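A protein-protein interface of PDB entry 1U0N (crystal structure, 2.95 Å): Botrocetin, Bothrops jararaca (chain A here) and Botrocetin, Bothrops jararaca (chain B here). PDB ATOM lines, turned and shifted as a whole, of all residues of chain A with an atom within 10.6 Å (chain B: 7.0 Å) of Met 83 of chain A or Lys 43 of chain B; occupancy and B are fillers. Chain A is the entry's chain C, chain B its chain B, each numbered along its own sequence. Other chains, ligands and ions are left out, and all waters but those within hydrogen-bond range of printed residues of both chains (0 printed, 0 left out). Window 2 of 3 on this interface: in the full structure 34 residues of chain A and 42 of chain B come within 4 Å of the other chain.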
ATOM      1  N   ARG A  76      -3.949  31.627 -13.525  1.00  0.00           N
ATOM      2  CA  ARG A  76      -5.228  31.246 -14.127  1.00  0.00           C
ATOM      3  C   ARG A  76      -4.837  30.248 -15.213  1.00  0.00           C
ATOM      4  O   ARG A  76      -4.192  30.624 -16.189  1.00  0.00           O
ATOM      5  CB  ARG A  76      -5.863  32.471 -14.774  1.00  0.00           C
ATOM      6  CG  ARG A  76      -7.374  32.503 -14.807  1.00  0.00           C
ATOM      7  CD  ARG A  76      -7.833  33.949 -14.984  1.00  0.00           C
ATOM      8  NE  ARG A  76      -9.190  34.165 -14.490  1.00  0.00           N
ATOM      9  CZ  ARG A  76      -9.595  33.884 -13.255  1.00  0.00           C
ATOM     10  NH1 ARG A  76      -8.747  33.372 -12.377  1.00  0.00           N
ATOM     11  NH2 ARG A  76     -10.853  34.111 -12.897  1.00  0.00           N
ATOM     12  N   PHE A  77      -5.225  28.987 -15.056  1.00  0.00           N
ATOM     13  CA  PHE A  77      -4.847  27.945 -16.015  1.00  0.00           C
ATOM     14  C   PHE A  77      -5.852  27.678 -17.127  1.00  0.00           C
ATOM     15  O   PHE A  77      -6.994  28.093 -17.048  1.00  0.00           O
ATOM     16  CB  PHE A  77      -4.577  26.637 -15.255  1.00  0.00           C
ATOM     17  CG  PHE A  77      -3.692  26.810 -14.050  1.00  0.00           C
ATOM     18  CD1 PHE A  77      -4.235  26.839 -12.772  1.00  0.00           C
ATOM     19  CD2 PHE A  77      -2.318  26.986 -14.196  1.00  0.00           C
ATOM     20  CE1 PHE A  77      -3.421  27.044 -11.659  1.00  0.00           C
ATOM     21  CE2 PHE A  77      -1.502  27.193 -13.088  1.00  0.00           C
ATOM     22  CZ  PHE A  77      -2.055  27.220 -11.818  1.00  0.00           C
ATOM     23  N   GLU A  78      -5.418  26.989 -18.173  1.00  0.00           N
ATOM     24  CA  GLU A  78      -6.318  26.638 -19.256  1.00  0.00           C
ATOM     25  C   GLU A  78      -5.785  25.492 -20.118  1.00  0.00           C
ATOM     26  O   GLU A  78      -4.574  25.327 -20.275  1.00  0.00           O
ATOM     27  CB  GLU A  78      -6.638  27.857 -20.129  1.00  0.00           C
ATOM     28  CG  GLU A  78      -5.476  28.484 -20.866  1.00  0.00           C
ATOM     29  CD  GLU A  78      -5.945  29.361 -22.027  1.00  0.00           C
ATOM     30  OE1 GLU A  78      -5.379  30.459 -22.223  1.00  0.00           O
ATOM     31  OE2 GLU A  78      -6.883  28.943 -22.751  1.00  0.00           O
ATOM     32  N   TRP A  79      -6.705  24.699 -20.666  1.00  0.00           N
ATOM     33  CA  TRP A  79      -6.365  23.553 -21.510  1.00  0.00           C
ATOM     34  C   TRP A  79      -6.475  23.902 -22.992  1.00  0.00           C
ATOM     35  O   TRP A  79      -7.511  24.362 -23.456  1.00  0.00           O
ATOM     36  CB  TRP A  79      -7.292  22.372 -21.191  1.00  0.00           C
ATOM     37  CG  TRP A  79      -7.205  21.903 -19.762  1.00  0.00           C
ATOM     38  CD1 TRP A  79      -7.866  22.413 -18.679  1.00  0.00           C
ATOM     39  CD2 TRP A  79      -6.370  20.858 -19.261  1.00  0.00           C
ATOM     40  NE1 TRP A  79      -7.492  21.749 -17.537  1.00  0.00           N
ATOM     41  CE2 TRP A  79      -6.574  20.790 -17.868  1.00  0.00           C
ATOM     42  CE3 TRP A  79      -5.464  19.969 -19.858  1.00  0.00           C
ATOM     43  CZ2 TRP A  79      -5.903  19.870 -17.063  1.00  0.00           C
ATOM     44  CZ3 TRP A  79      -4.799  19.057 -19.058  1.00  0.00           C
ATOM     45  CH2 TRP A  79      -5.021  19.015 -17.675  1.00  0.00           C
ATOM     46  N   THR A  80      -5.407  23.671 -23.738  1.00  0.00           N
ATOM     47  CA  THR A  80      -5.403  23.982 -25.160  1.00  0.00           C
ATOM     48  C   THR A  80      -6.627  23.446 -25.906  1.00  0.00           C
ATOM     49  O   THR A  80      -6.893  23.858 -27.036  1.00  0.00           O
ATOM     50  CB  THR A  80      -4.166  23.409 -25.839  1.00  0.00           C
ATOM     51  OG1 THR A  80      -4.229  21.981 -25.780  1.00  0.00           O
ATOM     52  CG2 THR A  80      -2.909  23.880 -25.145  1.00  0.00           C
ATOM     53  N   ASP A  81      -7.368  22.530 -25.289  1.00  0.00           N
ATOM     54  CA  ASP A  81      -8.543  21.949 -25.939  1.00  0.00           C
ATOM     55  C   ASP A  81      -9.840  22.521 -25.370  1.00  0.00           C
ATOM     56  O   ASP A  81     -10.930  22.002 -25.627  1.00  0.00           O
ATOM     57  CB  ASP A  81      -8.528  20.422 -25.777  1.00  0.00           C
ATOM     58  CG  ASP A  81      -9.211  19.951 -24.489  1.00  0.00           C
ATOM     59  OD1 ASP A  81      -9.135  20.659 -23.456  1.00  0.00           O
ATOM     60  OD2 ASP A  81      -9.817  18.855 -24.509  1.00  0.00           O
ATOM     61  N   GLY A  82      -9.716  23.582 -24.582  1.00  0.00           N
ATOM     62  CA  GLY A  82     -10.889  24.205 -24.008  1.00  0.00           C
ATOM     63  C   GLY A  82     -11.495  23.550 -22.780  1.00  0.00           C
ATOM     64  O   GLY A  82     -12.292  24.191 -22.098  1.00  0.00           O
ATOM     65  N   MET A  83     -11.130  22.302 -22.478  1.00  0.00           N
ATOM     66  CA  MET A  83     -11.689  21.593 -21.315  1.00  0.00           C
ATOM     67  C   MET A  83     -11.790  22.428 -20.047  1.00  0.00           C
ATOM     68  O   MET A  83     -10.769  22.814 -19.477  1.00  0.00           O
ATOM     69  CB  MET A  83     -10.867  20.346 -20.978  1.00  0.00           C
ATOM     70  CG  MET A  83     -11.044  19.920 -19.519  1.00  0.00           C
ATOM     71  SD  MET A  83     -10.137  18.474 -18.973  1.00  0.00           S
ATOM     72  CE  MET A  83     -11.451  17.269 -18.910  1.00  0.00           C
ATOM     73  N   GLU A  84     -13.006  22.685 -19.576  1.00  0.00           N
ATOM     74  CA  GLU A  84     -13.136  23.474 -18.363  1.00  0.00           C
ATOM     75  C   GLU A  84     -13.011  22.573 -17.145  1.00  0.00           C
ATOM     76  O   GLU A  84     -13.167  21.369 -17.241  1.00  0.00           O
ATOM     77  CB  GLU A  84     -14.460  24.260 -18.344  1.00  0.00           C
ATOM     78  CG  GLU A  84     -14.530  25.359 -17.238  1.00  0.00           C
ATOM     79  CD  GLU A  84     -13.219  26.167 -17.060  1.00  0.00           C
ATOM     80  OE1 GLU A  84     -12.755  26.798 -18.041  1.00  0.00           O
ATOM     81  OE2 GLU A  84     -12.659  26.168 -15.935  1.00  0.00           O
ATOM     82  N   PHE A  85     -12.724  23.170 -15.998  1.00  0.00           N
ATOM     83  CA  PHE A  85     -12.538  22.427 -14.766  1.00  0.00           C
ATOM     84  C   PHE A  85     -12.935  23.350 -13.625  1.00  0.00           C
ATOM     85  O   PHE A  85     -13.363  24.477 -13.867  1.00  0.00           O
ATOM     86  CB  PHE A  85     -11.067  22.085 -14.643  1.00  0.00           C
ATOM     87  CG  PHE A  85     -10.173  23.298 -14.699  1.00  0.00           C
ATOM     88  CD1 PHE A  85      -9.846  23.997 -13.540  1.00  0.00           C
ATOM     89  CD2 PHE A  85      -9.727  23.787 -15.919  1.00  0.00           C
ATOM     90  CE1 PHE A  85      -9.093  25.165 -13.600  1.00  0.00           C
ATOM     91  CE2 PHE A  85      -8.973  24.957 -15.987  1.00  0.00           C
ATOM     92  CZ  PHE A  85      -8.656  25.647 -14.826  1.00  0.00           C
ATOM     93  N   ASP A  86     -12.773  22.872 -12.390  1.00  0.00           N
ATOM     94  CA  ASP A  86     -13.085  23.648 -11.187  1.00  0.00           C
ATOM     95  C   ASP A  86     -11.834  23.831 -10.330  1.00  0.00           C
ATOM     96  O   ASP A  86     -11.341  22.880  -9.714  1.00  0.00           O
ATOM     97  CB  ASP A  86     -14.171  22.951 -10.359  1.00  0.00           C
ATOM     98  CG  ASP A  86     -14.318  23.538  -8.955  1.00  0.00           C
ATOM     99  OD1 ASP A  86     -15.282  23.163  -8.258  1.00  0.00           O
ATOM    100  OD2 ASP A  86     -13.481  24.363  -8.532  1.00  0.00           O
ATOM    101  N   TYR A  87     -11.342  25.066 -10.280  1.00  0.00           N
ATOM    102  CA  TYR A  87     -10.150  25.399  -9.512  1.00  0.00           C
ATOM    103  C   TYR A  87     -10.048  24.727  -8.156  1.00  0.00           C
ATOM    104  O   TYR A  87      -8.961  24.639  -7.588  1.00  0.00           O
ATOM    105  CB  TYR A  87     -10.038  26.907  -9.328  1.00  0.00           C
ATOM    106  CG  TYR A  87      -9.581  27.616 -10.569  1.00  0.00           C
ATOM    107  CD1 TYR A  87     -10.491  28.032 -11.532  1.00  0.00           C
ATOM    108  CD2 TYR A  87      -8.227  27.865 -10.788  1.00  0.00           C
ATOM    109  CE1 TYR A  87     -10.057  28.689 -12.690  1.00  0.00           C
ATOM    110  CE2 TYR A  87      -7.780  28.514 -11.931  1.00  0.00           C
ATOM    111  CZ  TYR A  87      -8.695  28.929 -12.879  1.00  0.00           C
ATOM    112  OH  TYR A  87      -8.267  29.606 -13.998  1.00  0.00           O
ATOM    113  N   ASP A  89     -10.606  21.536  -7.520  1.00  0.00           N
ATOM    114  CA  ASP A  89      -9.975  20.233  -7.701  1.00  0.00           C
ATOM    115  C   ASP A  89      -8.466  20.384  -7.904  1.00  0.00           C
ATOM    116  O   ASP A  89      -7.715  19.427  -7.735  1.00  0.00           O
ATOM    117  CB  ASP A  89     -10.584  19.490  -8.889  1.00  0.00           C
ATOM    118  CG  ASP A  89     -12.097  19.340  -8.780  1.00  0.00           C
ATOM    119  OD1 ASP A  89     -12.598  19.035  -7.676  1.00  0.00           O
ATOM    120  OD2 ASP A  89     -12.783  19.510  -9.818  1.00  0.00           O
ATOM    121  N   TYR A  90      -8.027  21.589  -8.258  1.00  0.00           N
ATOM    122  CA  TYR A  90      -6.607  21.846  -8.450  1.00  0.00           C
ATOM    123  C   TYR A  90      -5.937  22.366  -7.175  1.00  0.00           C
ATOM    124  O   TYR A  90      -5.709  23.571  -7.037  1.00  0.00           O
ATOM    125  CB  TYR A  90      -6.393  22.849  -9.588  1.00  0.00           C
ATOM    126  CG  TYR A  90      -6.761  22.315 -10.954  1.00  0.00           C
ATOM    127  CD1 TYR A  90      -6.541  23.069 -12.104  1.00  0.00           C
ATOM    128  CD2 TYR A  90      -7.357  21.065 -11.097  1.00  0.00           C
ATOM    129  CE1 TYR A  90      -6.913  22.588 -13.362  1.00  0.00           C
ATOM    130  CE2 TYR A  90      -7.726  20.585 -12.344  1.00  0.00           C
ATOM    131  CZ  TYR A  90      -7.504  21.346 -13.464  1.00  0.00           C
ATOM    132  OH  TYR A  90      -7.884  20.851 -14.686  1.00  0.00           O
ATOM    133  N   SER B  41      -5.714  16.251 -22.280  1.00  0.00           N
ATOM    134  CA  SER B  41      -6.330  16.972 -21.169  1.00  0.00           C
ATOM    135  C   SER B  41      -6.734  15.883 -20.167  1.00  0.00           C
ATOM    136  O   SER B  41      -7.341  14.883 -20.550  1.00  0.00           O
ATOM    137  CB  SER B  41      -7.556  17.744 -21.659  1.00  0.00           C
ATOM    138  OG  SER B  41      -8.338  16.951 -22.533  1.00  0.00           O
ATOM    139  N   ILE B  42      -6.394  16.065 -18.895  1.00  0.00           N
ATOM    140  CA  ILE B  42      -6.688  15.043 -17.902  1.00  0.00           C
ATOM    141  C   ILE B  42      -7.720  15.434 -16.860  1.00  0.00           C
ATOM    142  O   ILE B  42      -7.461  16.309 -16.025  1.00  0.00           O
ATOM    143  CB  ILE B  42      -5.434  14.644 -17.105  1.00  0.00           C
ATOM    144  CG1 ILE B  42      -4.192  14.603 -18.003  1.00  0.00           C
ATOM    145  CG2 ILE B  42      -5.689  13.311 -16.427  1.00  0.00           C
ATOM    146  CD1 ILE B  42      -4.237  13.575 -19.080  1.00  0.00           C
ATOM    147  N   LYS B  43      -8.870  14.766 -16.883  1.00  0.00           N
ATOM    148  CA  LYS B  43      -9.915  15.033 -15.906  1.00  0.00           C
ATOM    149  C   LYS B  43      -9.408  14.586 -14.533  1.00  0.00           C
ATOM    150  O   LYS B  43      -9.448  13.400 -14.199  1.00  0.00           O
ATOM    151  CB  LYS B  43     -11.182  14.272 -16.285  1.00  0.00           C
ATOM    152  CG  LYS B  43     -12.370  14.502 -15.372  1.00  0.00           C
ATOM    153  CD  LYS B  43     -13.644  14.028 -16.052  1.00  0.00           C
ATOM    154  CE  LYS B  43     -14.814  13.990 -15.083  1.00  0.00           C
ATOM    155  NZ  LYS B  43     -14.579  13.021 -13.973  1.00  0.00           N
ATOM    156  N   ILE B  44      -8.917  15.558 -13.761  1.00  0.00           N
ATOM    157  CA  ILE B  44      -8.356  15.359 -12.423  1.00  0.00           C
ATOM    158  C   ILE B  44      -8.804  14.119 -11.651  1.00  0.00           C
ATOM    159  O   ILE B  44      -7.972  13.396 -11.095  1.00  0.00           O
ATOM    160  CB  ILE B  44      -8.598  16.616 -11.568  1.00  0.00           C
ATOM    161  CG1 ILE B  44      -7.443  17.597 -11.757  1.00  0.00           C
ATOM    162  CG2 ILE B  44      -8.724  16.268 -10.119  1.00  0.00           C
ATOM    163  CD1 ILE B  44      -6.181  17.233 -11.018  1.00  0.00           C
ATOM    164  N   TYR B  45     -10.108  13.872 -11.594  1.00  0.00           N
ATOM    165  CA  TYR B  45     -10.599  12.699 -10.872  1.00  0.00           C
ATOM    166  C   TYR B  45     -11.366  11.761 -11.790  1.00  0.00           C
ATOM    167  O   TYR B  45     -12.587  11.875 -11.938  1.00  0.00           O
ATOM    168  CB  TYR B  45     -11.473  13.127  -9.683  1.00  0.00           C
ATOM    169  CG  TYR B  45     -10.735  14.022  -8.707  1.00  0.00           C
ATOM    170  CD1 TYR B  45      -9.434  13.709  -8.294  1.00  0.00           C
ATOM    171  CD2 TYR B  45     -11.312  15.201  -8.231  1.00  0.00           C
ATOM    172  CE1 TYR B  45      -8.725  14.550  -7.441  1.00  0.00           C
ATOM    173  CE2 TYR B  45     -10.612  16.050  -7.372  1.00  0.00           C
ATOM    174  CZ  TYR B  45      -9.318  15.720  -6.985  1.00  0.00           C
ATOM    175  OH  TYR B  45      -8.603  16.569  -6.167  1.00  0.00           O
ATOM    176  N   SER B  46     -10.639  10.835 -12.411  1.00  0.00           N
ATOM    177  CA  SER B  46     -11.247   9.869 -13.315  1.00  0.00           C
ATOM    178  C   SER B  46     -10.268   8.789 -13.784  1.00  0.00           C
ATOM    179  O   SER B  46      -9.050   8.935 -13.661  1.00  0.00           O
ATOM    180  CB  SER B  46     -11.842  10.597 -14.521  1.00  0.00           C
ATOM    181  OG  SER B  46     -10.918  11.524 -15.054  1.00  0.00           O
ATOM    182  N   LYS B  47     -10.815   7.698 -14.310  1.00  0.00           N
ATOM    183  CA  LYS B  47     -10.005   6.600 -14.808  1.00  0.00           C
ATOM    184  C   LYS B  47      -9.060   7.166 -15.865  1.00  0.00           C
ATOM    185  O   LYS B  47      -8.047   6.549 -16.190  1.00  0.00           O
ATOM    186  CB  LYS B  47     -10.905   5.525 -15.426  1.00  0.00           C
ATOM    187  CG  LYS B  47     -10.285   4.119 -15.570  1.00  0.00           C
ATOM    188  CD  LYS B  47      -9.069   4.035 -16.515  1.00  0.00           C
ATOM    189  CE  LYS B  47      -8.605   2.585 -16.679  1.00  0.00           C
ATOM    190  NZ  LYS B  47      -7.267   2.467 -17.312  1.00  0.00           N
ATOM    191  N   GLU B  48      -9.390   8.341 -16.397  1.00  0.00           N
ATOM    192  CA  GLU B  48      -8.546   8.973 -17.408  1.00  0.00           C
ATOM    193  C   GLU B  48      -7.137   9.245 -16.886  1.00  0.00           C
ATOM    194  O   GLU B  48      -6.159   9.076 -17.615  1.00  0.00           O
ATOM    195  CB  GLU B  48      -9.163  10.282 -17.895  1.00  0.00           C
ATOM    196  CG  GLU B  48      -8.208  11.087 -18.746  1.00  0.00           C
ATOM    197  CD  GLU B  48      -8.900  12.124 -19.593  1.00  0.00           C
ATOM    198  OE1 GLU B  48      -9.582  12.990 -19.019  1.00  0.00           O
ATOM    199  OE2 GLU B  48      -8.760  12.078 -20.835  1.00  0.00           O
ATOM    200  N   LYS B  49      -7.038   9.681 -15.631  1.00  0.00           N
ATOM    201  CA  LYS B  49      -5.743   9.949 -15.019  1.00  0.00           C
ATOM    202  C   LYS B  49      -4.931   8.680 -15.172  1.00  0.00           C
ATOM    203  O   LYS B  49      -3.845   8.691 -15.739  1.00  0.00           O
ATOM    204  CB  LYS B  49      -5.891  10.287 -13.532  1.00  0.00           C
ATOM    205  CG  LYS B  49      -4.553  10.461 -12.826  1.00  0.00           C
ATOM    206  CD  LYS B  49      -4.671  11.107 -11.446  1.00  0.00           C
ATOM    207  CE  LYS B  49      -5.204  10.156 -10.367  1.00  0.00           C
ATOM    208  NZ  LYS B  49      -4.326   8.975 -10.044  1.00  0.00           N
ATOM    209  N   LEU B  71      -2.629  21.361 -20.400  1.00  0.00           N
ATOM    210  CA  LEU B  71      -2.793  22.472 -19.475  1.00  0.00           C
ATOM    211  C   LEU B  71      -1.571  23.400 -19.420  1.00  0.00           C
ATOM    212  O   LEU B  71      -0.440  22.928 -19.497  1.00  0.00           O
ATOM    213  CB  LEU B  71      -3.057  21.912 -18.090  1.00  0.00           C
ATOM    214  CG  LEU B  71      -3.180  22.929 -16.967  1.00  0.00           C
ATOM    215  CD1 LEU B  71      -4.594  23.505 -16.948  1.00  0.00           C
ATOM    216  CD2 LEU B  71      -2.856  22.235 -15.650  1.00  0.00           C
ATOM    217  N   TRP B 115       0.867  16.097 -11.890  1.00  0.00           N
ATOM    218  CA  TRP B 115       1.231  17.185 -12.801  1.00  0.00           C
ATOM    219  C   TRP B 115       2.304  18.088 -12.218  1.00  0.00           C
ATOM    220  O   TRP B 115       2.469  18.179 -11.003  1.00  0.00           O
ATOM    221  CB  TRP B 115       0.037  18.089 -13.112  1.00  0.00           C
ATOM    222  CG  TRP B 115      -1.157  17.417 -13.627  1.00  0.00           C
ATOM    223  CD1 TRP B 115      -1.224  16.192 -14.211  1.00  0.00           C
ATOM    224  CD2 TRP B 115      -2.482  17.948 -13.651  1.00  0.00           C
ATOM    225  NE1 TRP B 115      -2.515  15.921 -14.600  1.00  0.00           N
ATOM    226  CE2 TRP B 115      -3.307  16.987 -14.271  1.00  0.00           C
ATOM    227  CE3 TRP B 115      -3.052  19.145 -13.212  1.00  0.00           C
ATOM    228  CZ2 TRP B 115      -4.672  17.185 -14.465  1.00  0.00           C
ATOM    229  CZ3 TRP B 115      -4.413  19.341 -13.403  1.00  0.00           C
ATOM    230  CH2 TRP B 115      -5.205  18.366 -14.024  1.00  0.00           C
ATOM    231  N   LYS B 129      -4.259  13.992 -27.704  1.00  0.00           N
ATOM    232  CA  LYS B 129      -5.610  13.495 -27.501  1.00  0.00           C
ATOM    233  C   LYS B 129      -6.402  14.123 -28.610  1.00  0.00           C
ATOM    234  O   LYS B 129      -6.151  15.266 -28.987  1.00  0.00           O
ATOM    235  CB  LYS B 129      -6.174  13.948 -26.156  1.00  0.00           C
ATOM    236  CG  LYS B 129      -7.585  13.459 -25.848  1.00  0.00           C
ATOM    237  CD  LYS B 129      -8.079  14.138 -24.572  1.00  0.00           C
ATOM    238  CE  LYS B 129      -9.327  13.489 -24.011  1.00  0.00           C
ATOM    239  NZ  LYS B 129      -9.456  13.784 -22.553  1.00  0.00           N
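The side-chain carboxylate (OD2) of Asp 81 of chain A is in hydrogen-bond range of the side-chain hydroxyl (OG) of Ser 41 of chain B (3.1 Å).
The side-chain hydroxyl (OH) of Tyr 45 of chain B sits at hydrogen-bond distance from the backbone carbonyl oxygen (O) of Asp 89 of chain A (3.4 Å).
The side-chain amino group (NZ) of Lys 129 of chain B sits at hydrogen-bond distance from the backbone carbonyl oxygen (O) of Ser 41 of chain B, 3.1 Å away.
O of Lys 43 of chain B is in hydrogen-bond range of OG of Ser 46 of chain B, at 2.5 Å.
The side-chain carboxylate (OE1) of Glu 48 of chain B lies within hydrogen-bond range of the backbone NH (N) of Lys 43 of chain B (2.9 Å).
The side-chain hydroxyl (OH) of Tyr 87 of chain A lies within hydrogen-bond range of the backbone NH (N) of Phe 77 of chain A, at 3.3 Å.
The side-chain hydroxyl (OH) of Tyr 90 of chain A sits at hydrogen-bond distance from the indole nitrogen (NE1) of Trp 79 of chain A (3.0 Å).
The side-chain carboxylate (OD1) of Asp 81 of chain A lies within hydrogen-bond range of the backbone NH (N) of Met 83 of chain A, 2.8 Å away.
Among the printed residues, merely in contact across the chains: Phe 77 of chain A with Leu 71 of chain B (3.6 Å), Glu 78 of chain A with Leu 71 of chain B (3.5 Å), Trp 79 of chain A with Ser 41 of chain B (3.3 Å), Trp 79 of chain A with Ile 42 of chain B (3.4 Å), Trp 79 of chain A with Leu 71 of chain B (3.2 Å), Trp 79 of chain A with Trp 115 of chain B (3.5 Å), Met 83 of chain A with Ser 41 of chain B (3.8 Å), Met 83 of chain A with Lys 43 of chain B (3.99 Å), Asp 89 of chain A with Ile 44 of chain B (3.9 Å), Tyr 90 of chain A with Ile 44 of chain B (3.1 Å) and Tyr 90 of chain A with Trp 115 of chain B (3.7 Å).
Of the printed residues of chain B, Trp 79 of chain A touches Ser 41, Ile 42, Leu 71 and Trp 115.
No residue of chain B comes within 4 Å of Gly 82 of chain A.
Printed residues of chain B within 4 Å of Met 83 of chain A: Ser 41 (3.8 Å) and Lys 43 (3.99 Å).
Glu 84 of chain A touches none of the printed residues of chain B.
Ser 41 of chain B touches just these residues of chain A: Trp 79 (3.3 Å), Asp 81 (3.1 Å) and Met 83 (3.8 Å).
Ile 42 of chain B touches one residue of chain A.
Printed residues of chain A within 4 Å of Lys 43 of chain B: Met 83.
Of chain A, only Asp 89 and Tyr 90 come within 4 Å of Ile 44 of chain B.
Printed residues of chain A within 4 Å of Tyr 45 of chain B: Asp 89 (3.4 Å).
Lys 47 of chain B touches none of the printed residues of chain A.
The nearest printed residue of chain A that does not touch Lys 43 of chain B is Trp 79 of chain A (5.8 Å).
Hydrophobic or aromatic side chains of chain B within 4 Å of the printed part of chain A: Ile 44, Tyr 45, Leu 71 and Trp 115.
Printed residues of chain A that touch a printed residue of chain B: Phe 77, Glu 78, Trp 79, Asp 81, Met 83, Asp 89 and Tyr 90.
Hydrophobic or aromatic side chains of chain A within 4 Å of the printed part of chain B: Phe 77, Trp 79, Met 83 and Tyr 90.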
